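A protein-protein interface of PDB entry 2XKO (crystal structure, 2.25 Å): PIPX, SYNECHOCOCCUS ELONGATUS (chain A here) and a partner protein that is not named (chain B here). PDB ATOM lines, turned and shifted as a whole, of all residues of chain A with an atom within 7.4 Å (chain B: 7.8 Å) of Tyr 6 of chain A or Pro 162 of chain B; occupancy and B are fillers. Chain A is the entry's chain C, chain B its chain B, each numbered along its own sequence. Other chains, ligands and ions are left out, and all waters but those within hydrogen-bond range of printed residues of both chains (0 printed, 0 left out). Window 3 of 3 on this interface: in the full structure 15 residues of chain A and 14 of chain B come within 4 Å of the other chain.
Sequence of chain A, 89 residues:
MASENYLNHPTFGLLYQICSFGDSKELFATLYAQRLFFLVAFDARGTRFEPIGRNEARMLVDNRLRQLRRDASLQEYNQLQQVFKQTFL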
ATOM      1  N   GLU A   4      13.287  18.137   5.560  1.00  0.00           N
ATOM      2  CA  GLU A   4      14.231  18.442   6.709  1.00  0.00           C
ATOM      3  C   GLU A   4      15.640  17.805   6.587  1.00  0.00           C
ATOM      4  O   GLU A   4      16.442  17.889   7.523  1.00  0.00           O
ATOM      5  CB  GLU A   4      13.598  18.093   8.078  1.00  0.00           C
ATOM      6  CG  GLU A   4      13.739  16.610   8.524  1.00  0.00           C
ATOM      7  CD  GLU A   4      13.976  16.425  10.022  1.00  0.00           C
ATOM      8  OE1 GLU A   4      13.915  17.406  10.794  1.00  0.00           O
ATOM      9  OE2 GLU A   4      14.217  15.271  10.436  1.00  0.00           O
ATOM     10  N   ASN A   5      15.919  17.154   5.459  1.00  0.00           N
ATOM     11  CA  ASN A   5      17.283  16.869   5.016  1.00  0.00           C
ATOM     12  C   ASN A   5      17.663  17.948   3.966  1.00  0.00           C
ATOM     13  O   ASN A   5      16.813  18.408   3.207  1.00  0.00           O
ATOM     14  CB  ASN A   5      17.361  15.445   4.468  1.00  0.00           C
ATOM     15  CG  ASN A   5      18.531  15.225   3.509  1.00  0.00           C
ATOM     16  OD1 ASN A   5      19.699  15.334   3.881  1.00  0.00           O
ATOM     17  ND2 ASN A   5      18.212  14.853   2.274  1.00  0.00           N
ATOM     18  N   TYR A   6      18.935  18.343   3.947  1.00  0.00           N
ATOM     19  CA  TYR A   6      19.388  19.548   3.270  1.00  0.00           C
ATOM     20  C   TYR A   6      20.574  19.317   2.339  1.00  0.00           C
ATOM     21  O   TYR A   6      21.310  18.342   2.476  1.00  0.00           O
ATOM     22  CB  TYR A   6      19.797  20.569   4.309  1.00  0.00           C
ATOM     23  CG  TYR A   6      18.685  21.041   5.196  1.00  0.00           C
ATOM     24  CD1 TYR A   6      17.879  22.089   4.797  1.00  0.00           C
ATOM     25  CD2 TYR A   6      18.468  20.478   6.462  1.00  0.00           C
ATOM     26  CE1 TYR A   6      16.867  22.564   5.598  1.00  0.00           C
ATOM     27  CE2 TYR A   6      17.450  20.947   7.296  1.00  0.00           C
ATOM     28  CZ  TYR A   6      16.648  21.999   6.848  1.00  0.00           C
ATOM     29  OH  TYR A   6      15.625  22.519   7.606  1.00  0.00           O
ATOM     30  N   LEU A   7      20.767  20.241   1.404  1.00  0.00           N
ATOM     31  CA  LEU A   7      21.796  20.109   0.383  1.00  0.00           C
ATOM     32  C   LEU A   7      22.124  21.474  -0.226  1.00  0.00           C
ATOM     33  O   LEU A   7      21.219  22.248  -0.585  1.00  0.00           O
ATOM     34  CB  LEU A   7      21.283  19.196  -0.723  1.00  0.00           C
ATOM     35  CG  LEU A   7      22.297  18.458  -1.589  1.00  0.00           C
ATOM     36  CD1 LEU A   7      22.955  17.312  -0.790  1.00  0.00           C
ATOM     37  CD2 LEU A   7      21.585  17.926  -2.840  1.00  0.00           C
ATOM     38  N   ASN A   8      23.410  21.741  -0.389  1.00  0.00           N
ATOM     39  CA  ASN A   8      23.854  23.027  -0.904  1.00  0.00           C
ATOM     40  C   ASN A   8      24.048  22.976  -2.396  1.00  0.00           C
ATOM     41  O   ASN A   8      24.939  22.292  -2.867  1.00  0.00           O
ATOM     42  CB  ASN A   8      25.171  23.440  -0.235  1.00  0.00           C
ATOM     43  CG  ASN A   8      25.093  24.811   0.411  1.00  0.00           C
ATOM     44  OD1 ASN A   8      24.137  25.562   0.192  1.00  0.00           O
ATOM     45  ND2 ASN A   8      26.086  25.129   1.245  1.00  0.00           N
ATOM     46  N   LEU A  14      21.082  26.826  -0.077  1.00  0.00           N
ATOM     47  CA  LEU A  14      20.539  25.691   0.675  1.00  0.00           C
ATOM     48  C   LEU A  14      19.218  25.197   0.086  1.00  0.00           C
ATOM     49  O   LEU A  14      18.300  25.972  -0.193  1.00  0.00           O
ATOM     50  CB  LEU A  14      20.358  26.082   2.144  1.00  0.00           C
ATOM     51  CG  LEU A  14      20.472  24.985   3.193  1.00  0.00           C
ATOM     52  CD1 LEU A  14      21.818  24.277   3.126  1.00  0.00           C
ATOM     53  CD2 LEU A  14      20.256  25.611   4.547  1.00  0.00           C
ATOM     54  N   LEU A  15      19.142  23.892  -0.128  1.00  0.00           N
ATOM     55  CA  LEU A  15      17.911  23.251  -0.596  1.00  0.00           C
ATOM     56  C   LEU A  15      17.446  22.281   0.482  1.00  0.00           C
ATOM     57  O   LEU A  15      18.247  21.870   1.319  1.00  0.00           O
ATOM     58  CB  LEU A  15      18.183  22.519  -1.899  1.00  0.00           C
ATOM     59  CG  LEU A  15      18.876  23.332  -3.004  1.00  0.00           C
ATOM     60  CD1 LEU A  15      19.234  22.391  -4.158  1.00  0.00           C
ATOM     61  CD2 LEU A  15      18.012  24.512  -3.492  1.00  0.00           C
ATOM     62  N   TYR A  16      16.151  21.948   0.486  1.00  0.00           N
ATOM     63  CA  TYR A  16      15.627  20.908   1.388  1.00  0.00           C
ATOM     64  C   TYR A  16      14.859  19.862   0.607  1.00  0.00           C
ATOM     65  O   TYR A  16      14.245  20.164  -0.408  1.00  0.00           O
ATOM     66  CB  TYR A  16      14.761  21.491   2.515  1.00  0.00           C
ATOM     67  CG  TYR A  16      13.404  21.937   2.068  1.00  0.00           C
ATOM     68  CD1 TYR A  16      13.234  23.135   1.361  1.00  0.00           C
ATOM     69  CD2 TYR A  16      12.273  21.167   2.343  1.00  0.00           C
ATOM     70  CE1 TYR A  16      11.978  23.541   0.925  1.00  0.00           C
ATOM     71  CE2 TYR A  16      11.010  21.580   1.921  1.00  0.00           C
ATOM     72  CZ  TYR A  16      10.873  22.763   1.209  1.00  0.00           C
ATOM     73  OH  TYR A  16       9.620  23.169   0.812  1.00  0.00           O
ATOM     74  N   GLN A  17      14.905  18.630   1.104  1.00  0.00           N
ATOM     75  CA  GLN A  17      14.344  17.492   0.407  1.00  0.00           C
ATOM     76  C   GLN A  17      12.859  17.458   0.577  1.00  0.00           C
ATOM     77  O   GLN A  17      12.367  17.630   1.654  1.00  0.00           O
ATOM     78  CB  GLN A  17      14.935  16.199   0.952  1.00  0.00           C
ATOM     79  CG  GLN A  17      14.557  14.981   0.142  1.00  0.00           C
ATOM     80  CD  GLN A  17      14.695  13.705   0.922  1.00  0.00           C
ATOM     81  OE1 GLN A  17      14.411  13.677   2.110  1.00  0.00           O
ATOM     82  NE2 GLN A  17      15.131  12.641   0.263  1.00  0.00           N
ATOM     83  N   GLU A  26      16.284  12.089  -5.957  1.00  0.00           N
ATOM     84  CA  GLU A  26      15.519  12.830  -4.930  1.00  0.00           C
ATOM     85  C   GLU A  26      14.983  14.152  -5.455  1.00  0.00           C
ATOM     86  O   GLU A  26      15.585  14.747  -6.348  1.00  0.00           O
ATOM     87  CB  GLU A  26      16.407  13.118  -3.711  1.00  0.00           C
ATOM     88  CG  GLU A  26      17.124  11.865  -3.174  1.00  0.00           C
ATOM     89  CD  GLU A  26      17.416  11.923  -1.695  1.00  0.00           C
ATOM     90  OE1 GLU A  26      18.132  12.845  -1.262  1.00  0.00           O
ATOM     91  OE2 GLU A  26      16.929  11.035  -0.955  1.00  0.00           O
ATOM     92  N   PHE A  28      14.243  18.035  -4.424  1.00  0.00           N
ATOM     93  CA  PHE A  28      14.609  19.077  -3.461  1.00  0.00           C
ATOM     94  C   PHE A  28      13.953  20.412  -3.863  1.00  0.00           C
ATOM     95  O   PHE A  28      13.492  20.570  -4.998  1.00  0.00           O
ATOM     96  CB  PHE A  28      16.128  19.242  -3.434  1.00  0.00           C
ATOM     97  CG  PHE A  28      16.845  18.299  -2.484  1.00  0.00           C
ATOM     98  CD1 PHE A  28      17.342  18.750  -1.269  1.00  0.00           C
ATOM     99  CD2 PHE A  28      17.050  16.970  -2.817  1.00  0.00           C
ATOM    100  CE1 PHE A  28      18.001  17.877  -0.401  1.00  0.00           C
ATOM    101  CE2 PHE A  28      17.719  16.104  -1.961  1.00  0.00           C
ATOM    102  CZ  PHE A  28      18.191  16.554  -0.759  1.00  0.00           C
ATOM    103  N   ALA A  29      13.945  21.391  -2.967  1.00  0.00           N
ATOM    104  CA  ALA A  29      13.380  22.673  -3.304  1.00  0.00           C
ATOM    105  C   ALA A  29      14.145  23.775  -2.593  1.00  0.00           C
ATOM    106  O   ALA A  29      14.819  23.530  -1.581  1.00  0.00           O
ATOM    107  CB  ALA A  29      11.906  22.729  -2.942  1.00  0.00           C
ATOM    108  N   LEU A  31      14.861  26.893  -0.252  1.00  0.00           N
ATOM    109  CA  LEU A  31      14.424  27.198   1.099  1.00  0.00           C
ATOM    110  C   LEU A  31      13.447  28.361   1.093  1.00  0.00           C
ATOM    111  O   LEU A  31      12.439  28.318   1.785  1.00  0.00           O
ATOM    112  CB  LEU A  31      15.639  27.539   1.957  1.00  0.00           C
ATOM    113  CG  LEU A  31      15.519  27.270   3.442  1.00  0.00           C
ATOM    114  CD1 LEU A  31      15.411  25.762   3.690  1.00  0.00           C
ATOM    115  CD2 LEU A  31      16.728  27.840   4.141  1.00  0.00           C
ATOM    116  N   PHE A  42      22.583  11.177  -7.377  1.00  0.00           N
ATOM    117  CA  PHE A  42      23.876  10.968  -6.718  1.00  0.00           C
ATOM    118  C   PHE A  42      24.635   9.806  -7.343  1.00  0.00           C
ATOM    119  O   PHE A  42      24.024   8.878  -7.880  1.00  0.00           O
ATOM    120  CB  PHE A  42      23.688  10.658  -5.237  1.00  0.00           C
ATOM    121  CG  PHE A  42      22.834  11.655  -4.496  1.00  0.00           C
ATOM    122  CD1 PHE A  42      23.310  12.934  -4.232  1.00  0.00           C
ATOM    123  CD2 PHE A  42      21.580  11.294  -4.020  1.00  0.00           C
ATOM    124  CE1 PHE A  42      22.540  13.848  -3.525  1.00  0.00           C
ATOM    125  CE2 PHE A  42      20.801  12.205  -3.313  1.00  0.00           C
ATOM    126  CZ  PHE A  42      21.280  13.486  -3.066  1.00  0.00           C
ATOM    127  N   CYS B 156      19.939  32.174   5.830  1.00  0.00           N
ATOM    128  CA  CYS B 156      19.825  30.718   5.910  1.00  0.00           C
ATOM    129  C   CYS B 156      20.137  30.077   4.547  1.00  0.00           C
ATOM    130  O   CYS B 156      20.840  29.075   4.476  1.00  0.00           O
ATOM    131  CB  CYS B 156      18.425  30.263   6.364  1.00  0.00           C
ATOM    132  SG  CYS B 156      18.038  30.671   8.015  1.00  0.00           S
ATOM    133  N   PHE B 159      24.141  31.056   3.808  1.00  0.00           N
ATOM    134  CA  PHE B 159      25.156  30.711   4.783  1.00  0.00           C
ATOM    135  C   PHE B 159      24.705  29.704   5.841  1.00  0.00           C
ATOM    136  O   PHE B 159      25.424  29.485   6.804  1.00  0.00           O
ATOM    137  CB  PHE B 159      25.621  31.975   5.515  1.00  0.00           C
ATOM    138  CG  PHE B 159      26.103  33.028   4.610  1.00  0.00           C
ATOM    139  CD1 PHE B 159      27.377  32.956   4.058  1.00  0.00           C
ATOM    140  CD2 PHE B 159      25.278  34.086   4.248  1.00  0.00           C
ATOM    141  CE1 PHE B 159      27.827  33.952   3.152  1.00  0.00           C
ATOM    142  CE2 PHE B 159      25.731  35.083   3.354  1.00  0.00           C
ATOM    143  CZ  PHE B 159      26.987  35.013   2.812  1.00  0.00           C
ATOM    144  N   GLY B 160      23.550  29.080   5.669  1.00  0.00           N
ATOM    145  CA  GLY B 160      22.989  28.232   6.717  1.00  0.00           C
ATOM    146  C   GLY B 160      23.584  26.843   6.800  1.00  0.00           C
ATOM    147  O   GLY B 160      24.011  26.322   5.790  1.00  0.00           O
ATOM    148  N   ILE B 161      23.613  26.273   8.017  1.00  0.00           N
ATOM    149  CA  ILE B 161      24.080  24.900   8.291  1.00  0.00           C
ATOM    150  C   ILE B 161      22.951  24.169   9.030  1.00  0.00           C
ATOM    151  O   ILE B 161      22.343  24.721   9.954  1.00  0.00           O
ATOM    152  CB  ILE B 161      25.366  24.877   9.210  1.00  0.00           C
ATOM    153  CG1 ILE B 161      26.460  25.732   8.620  1.00  0.00           C
ATOM    154  CG2 ILE B 161      25.977  23.470   9.360  1.00  0.00           C
ATOM    155  CD1 ILE B 161      26.739  25.467   7.138  1.00  0.00           C
ATOM    156  N   PRO B 162      22.662  22.920   8.641  1.00  0.00           N
ATOM    157  CA  PRO B 162      21.703  22.189   9.449  1.00  0.00           C
ATOM    158  C   PRO B 162      22.244  21.992  10.848  1.00  0.00           C
ATOM    159  O   PRO B 162      23.438  21.816  11.035  1.00  0.00           O
ATOM    160  CB  PRO B 162      21.561  20.847   8.728  1.00  0.00           C
ATOM    161  CG  PRO B 162      22.038  21.103   7.354  1.00  0.00           C
ATOM    162  CD  PRO B 162      23.082  22.165   7.459  1.00  0.00           C
ATOM    163  N   SER B 163      21.372  22.097  11.831  1.00  0.00           N
ATOM    164  CA  SER B 163      21.811  22.016  13.201  1.00  0.00           C
ATOM    165  C   SER B 163      20.659  21.402  13.974  1.00  0.00           C
ATOM    166  O   SER B 163      19.521  21.342  13.474  1.00  0.00           O
ATOM    167  CB  SER B 163      22.247  23.403  13.742  1.00  0.00           C
ATOM    168  OG  SER B 163      21.130  24.210  14.111  1.00  0.00           O
ATOM    169  N   PRO B 164      20.946  20.904  15.180  1.00  0.00           N
ATOM    170  CA  PRO B 164      19.894  20.104  15.823  1.00  0.00           C
ATOM    171  C   PRO B 164      18.503  20.776  15.783  1.00  0.00           C
ATOM    172  O   PRO B 164      17.497  20.120  15.478  1.00  0.00           O
ATOM    173  CB  PRO B 164      20.442  19.919  17.244  1.00  0.00           C
ATOM    174  CG  PRO B 164      21.966  19.834  17.040  1.00  0.00           C
ATOM    175  CD  PRO B 164      22.219  20.889  15.949  1.00  0.00           C
ATOM    176  N   ASP B 165      18.495  22.092  15.978  1.00  0.00           N
ATOM    177  CA  ASP B 165      17.289  22.880  16.197  1.00  0.00           C
ATOM    178  C   ASP B 165      16.698  23.534  14.916  1.00  0.00           C
ATOM    179  O   ASP B 165      15.524  23.942  14.888  1.00  0.00           O
ATOM    180  CB  ASP B 165      17.613  23.942  17.259  1.00  0.00           C
ATOM    181  CG  ASP B 165      17.910  23.327  18.630  1.00  0.00           C
ATOM    182  OD1 ASP B 165      18.536  22.238  18.705  1.00  0.00           O
ATOM    183  OD2 ASP B 165      17.507  23.924  19.647  1.00  0.00           O
ATOM    184  N   GLY B 166      17.495  23.640  13.856  1.00  0.00           N
ATOM    185  CA  GLY B 166      16.975  24.133  12.581  1.00  0.00           C
ATOM    186  C   GLY B 166      18.108  24.423  11.615  1.00  0.00           C
ATOM    187  O   GLY B 166      18.961  23.563  11.365  1.00  0.00           O
ATOM    188  N   ILE B 167      18.123  25.636  11.076  1.00  0.00           N
ATOM    189  CA  ILE B 167      19.241  26.102  10.296  1.00  0.00           C
ATOM    190  C   ILE B 167      19.913  27.208  11.101  1.00  0.00           C
ATOM    191  O   ILE B 167      19.261  28.150  11.553  1.00  0.00           O
ATOM    192  CB  ILE B 167      18.821  26.620   8.900  1.00  0.00           C
ATOM    193  CG1 ILE B 167      18.115  25.525   8.101  1.00  0.00           C
ATOM    194  CG2 ILE B 167      20.036  27.122   8.112  1.00  0.00           C
ATOM    195  CD1 ILE B 167      18.924  24.240   7.950  1.00  0.00           C
ATOM    196  N   THR B 168      21.213  27.069  11.263  1.00  0.00           N
ATOM    197  CA  THR B 168      22.052  28.018  11.929  1.00  0.00           C
ATOM    198  C   THR B 168      22.724  28.794  10.849  1.00  0.00           C
ATOM    199  O   THR B 168      23.312  28.206   9.952  1.00  0.00           O
ATOM    200  CB  THR B 168      23.167  27.278  12.775  1.00  0.00           C
ATOM    201  OG1 THR B 168      22.540  26.451  13.744  1.00  0.00           O
ATOM    202  CG2 THR B 168      24.072  28.268  13.475  1.00  0.00           C
ATOM    203  N   ILE B 169      22.632  30.106  10.920  1.00  0.00           N
ATOM    204  CA  ILE B 169      23.291  30.973   9.971  1.00  0.00           C
ATOM    205  C   ILE B 169      24.764  31.017  10.351  1.00  0.00           C
ATOM    206  O   ILE B 169      25.130  31.545  11.419  1.00  0.00           O
ATOM    207  CB  ILE B 169      22.729  32.379  10.021  1.00  0.00           C
ATOM    208  CG1 ILE B 169      21.304  32.421   9.445  1.00  0.00           C
ATOM    209  CG2 ILE B 169      23.586  33.293   9.230  1.00  0.00           C
ATOM    210  CD1 ILE B 169      20.464  33.632   9.973  1.00  0.00           C
ATOM    211  N   THR B 210      20.077  30.876  14.962  1.00  0.00           N
ATOM    212  CA  THR B 210      19.505  29.645  14.453  1.00  0.00           C
ATOM    213  C   THR B 210      18.046  29.926  14.229  1.00  0.00           C
ATOM    214  O   THR B 210      17.385  30.419  15.133  1.00  0.00           O
ATOM    215  CB  THR B 210      19.687  28.505  15.490  1.00  0.00           C
ATOM    216  OG1 THR B 210      21.085  28.200  15.599  1.00  0.00           O
ATOM    217  CG2 THR B 210      18.885  27.210  15.097  1.00  0.00           C
ATOM    218  N   VAL B 211      17.557  29.640  13.015  1.00  0.00           N
ATOM    219  CA  VAL B 211      16.143  29.783  12.662  1.00  0.00           C
ATOM    220  C   VAL B 211      15.507  28.390  12.675  1.00  0.00           C
ATOM    221  O   VAL B 211      15.925  27.497  11.910  1.00  0.00           O
ATOM    222  CB  VAL B 211      15.970  30.417  11.275  1.00  0.00           C
ATOM    223  CG1 VAL B 211      14.478  30.395  10.847  1.00  0.00           C
ATOM    224  CG2 VAL B 211      16.527  31.846  11.270  1.00  0.00           C
ATOM    225  N   PHE B 212      14.506  28.204  13.533  1.00  0.00           N
ATOM    226  CA  PHE B 212      14.051  26.867  13.863  1.00  0.00           C
ATOM    227  C   PHE B 212      13.344  26.149  12.713  1.00  0.00           C
ATOM    228  O   PHE B 212      13.559  24.941  12.521  1.00  0.00           O
ATOM    229  CB  PHE B 212      13.092  26.872  15.059  1.00  0.00           C
ATOM    230  CG  PHE B 212      13.711  27.275  16.375  1.00  0.00           C
ATOM    231  CD1 PHE B 212      15.007  26.897  16.726  1.00  0.00           C
ATOM    232  CD2 PHE B 212      12.939  27.975  17.306  1.00  0.00           C
ATOM    233  CE1 PHE B 212      15.540  27.265  17.958  1.00  0.00           C
ATOM    234  CE2 PHE B 212      13.452  28.348  18.545  1.00  0.00           C
ATOM    235  CZ  PHE B 212      14.750  27.985  18.882  1.00  0.00           C
ATOM    236  N   ASN B 213      12.454  26.854  12.019  1.00  0.00           N
ATOM    237  CA  ASN B 213      11.706  26.257  10.923  1.00  0.00           C
ATOM    238  C   ASN B 213      11.675  27.204   9.742  1.00  0.00           C
ATOM    239  O   ASN B 213      10.620  27.746   9.416  1.00  0.00           O
ATOM    240  CB  ASN B 213      10.264  25.954  11.331  1.00  0.00           C
ATOM    241  CG  ASN B 213      10.135  24.676  12.067  1.00  0.00           C
ATOM    242  OD1 ASN B 213       9.695  23.654  11.501  1.00  0.00           O
ATOM    243  ND2 ASN B 213      10.524  24.691  13.344  1.00  0.00           N
ATOM    244  N   PRO B 214      12.825  27.402   9.095  1.00  0.00           N
ATOM    245  CA  PRO B 214      12.906  28.388   8.002  1.00  0.00           C
ATOM    246  C   PRO B 214      11.940  28.117   6.836  1.00  0.00           C
ATOM    247  O   PRO B 214      11.455  29.065   6.231  1.00  0.00           O
ATOM    248  CB  PRO B 214      14.365  28.328   7.576  1.00  0.00           C
ATOM    249  CG  PRO B 214      14.876  26.989   8.119  1.00  0.00           C
ATOM    250  CD  PRO B 214      14.085  26.673   9.304  1.00  0.00           C
ATOM    251  N   VAL B 215      11.626  26.851   6.558  1.00  0.00           N
ATOM    252  CA  VAL B 215      10.671  26.519   5.503  1.00  0.00           C
ATOM    253  C   VAL B 215       9.305  27.066   5.853  1.00  0.00           C
ATOM    254  O   VAL B 215       8.710  27.804   5.055  1.00  0.00           O
ATOM    255  CB  VAL B 215      10.583  25.008   5.253  1.00  0.00           C
ATOM    256  CG1 VAL B 215       9.387  24.662   4.356  1.00  0.00           C
ATOM    257  CG2 VAL B 215      11.863  24.527   4.627  1.00  0.00           C
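Hydrophobic or aromatic side chains of chain B within 4 Å of the printed part of chain A: Pro 162, Ile 167 and Val 215.
Along chain B the printed residues that touch a printed residue of chain A span positions 156 to 215.
Of the 14 printed residues of chain A, 4 touch a printed residue of chain B.
Along chain A the printed residues that touch a printed residue of chain B span positions 6 to 31.
Among the printed residues, no Asp or Glu carboxylate lies within 4 Å of a Lys or Arg side-chain nitrogen of the other chain.
The backbone carbonyl oxygen (O) of Ile 167 of chain B is in hydrogen-bond range of the backbone NH (N) of Val 211 of chain B (2.7 Å).
The backbone carbonyl oxygen (O) of Tyr 16 of chain A sits at hydrogen-bond distance from the backbone NH (N) of Ala 29 of chain A.
The side-chain amide oxygen of Asn 8 of chain A is in hydrogen-bond range of the backbone NH of Leu 14 of chain A (3.3 Å).
Tyr 6 of chain A touches Pro 162 of chain B.
CZ of Tyr 6 of chain A touches CD1 of Ile 167 of chain B, 3.4 Å away.
O of Cys 156 of chain B touches CD2 of Leu 14 of chain A (3.5 Å).
Leu 14 of chain A touches Ile 167 of chain B (CD2 to CG2, 3.9 Å).
CD1 of Tyr 16 of chain A touches CG2 of Val 215 of chain B (3.8 Å).
CB of Cys 156 of chain B touches CD2 of Leu 31 of chain A, 3.7 Å away.
Leu 31 of chain A touches Val 215 of chain B.
Tyr 6 of chain A touches just these residues of chain B: Pro 162 and Ile 167.
Of the printed residues of chain B, Tyr 16 of chain A touches Val 215 (3.8 Å).
Printed residues of chain B within 4 Å of Leu 31 of chain A: Cys 156 (3.7 Å) and Val 215 (3.9 Å).
Printed residues of chain A within 4 Å of Cys 156 of chain B: Leu 14 and Leu 31.
Of chain A, only Tyr 6 comes within 4 Å of Pro 162 of chain B.
Of the printed residues of chain A, Ile 167 of chain B touches Tyr 6 (3.4 Å) and Leu 14 (3.9 Å).
Of the printed residues of chain A, Val 215 of chain B touches Tyr 16 and Leu 31.
The nearest residue of chain B that does not touch Tyr 6 of chain A is Pro 214 of chain B (4.6 Å).
The nearest residue of chain A that does not touch Pro 162 of chain B is Leu 14 of chain A (5.0 Å).
The nearest printed residue of chain A that does not touch Val 215 of chain B is Tyr 6 of chain A (5.2 Å).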
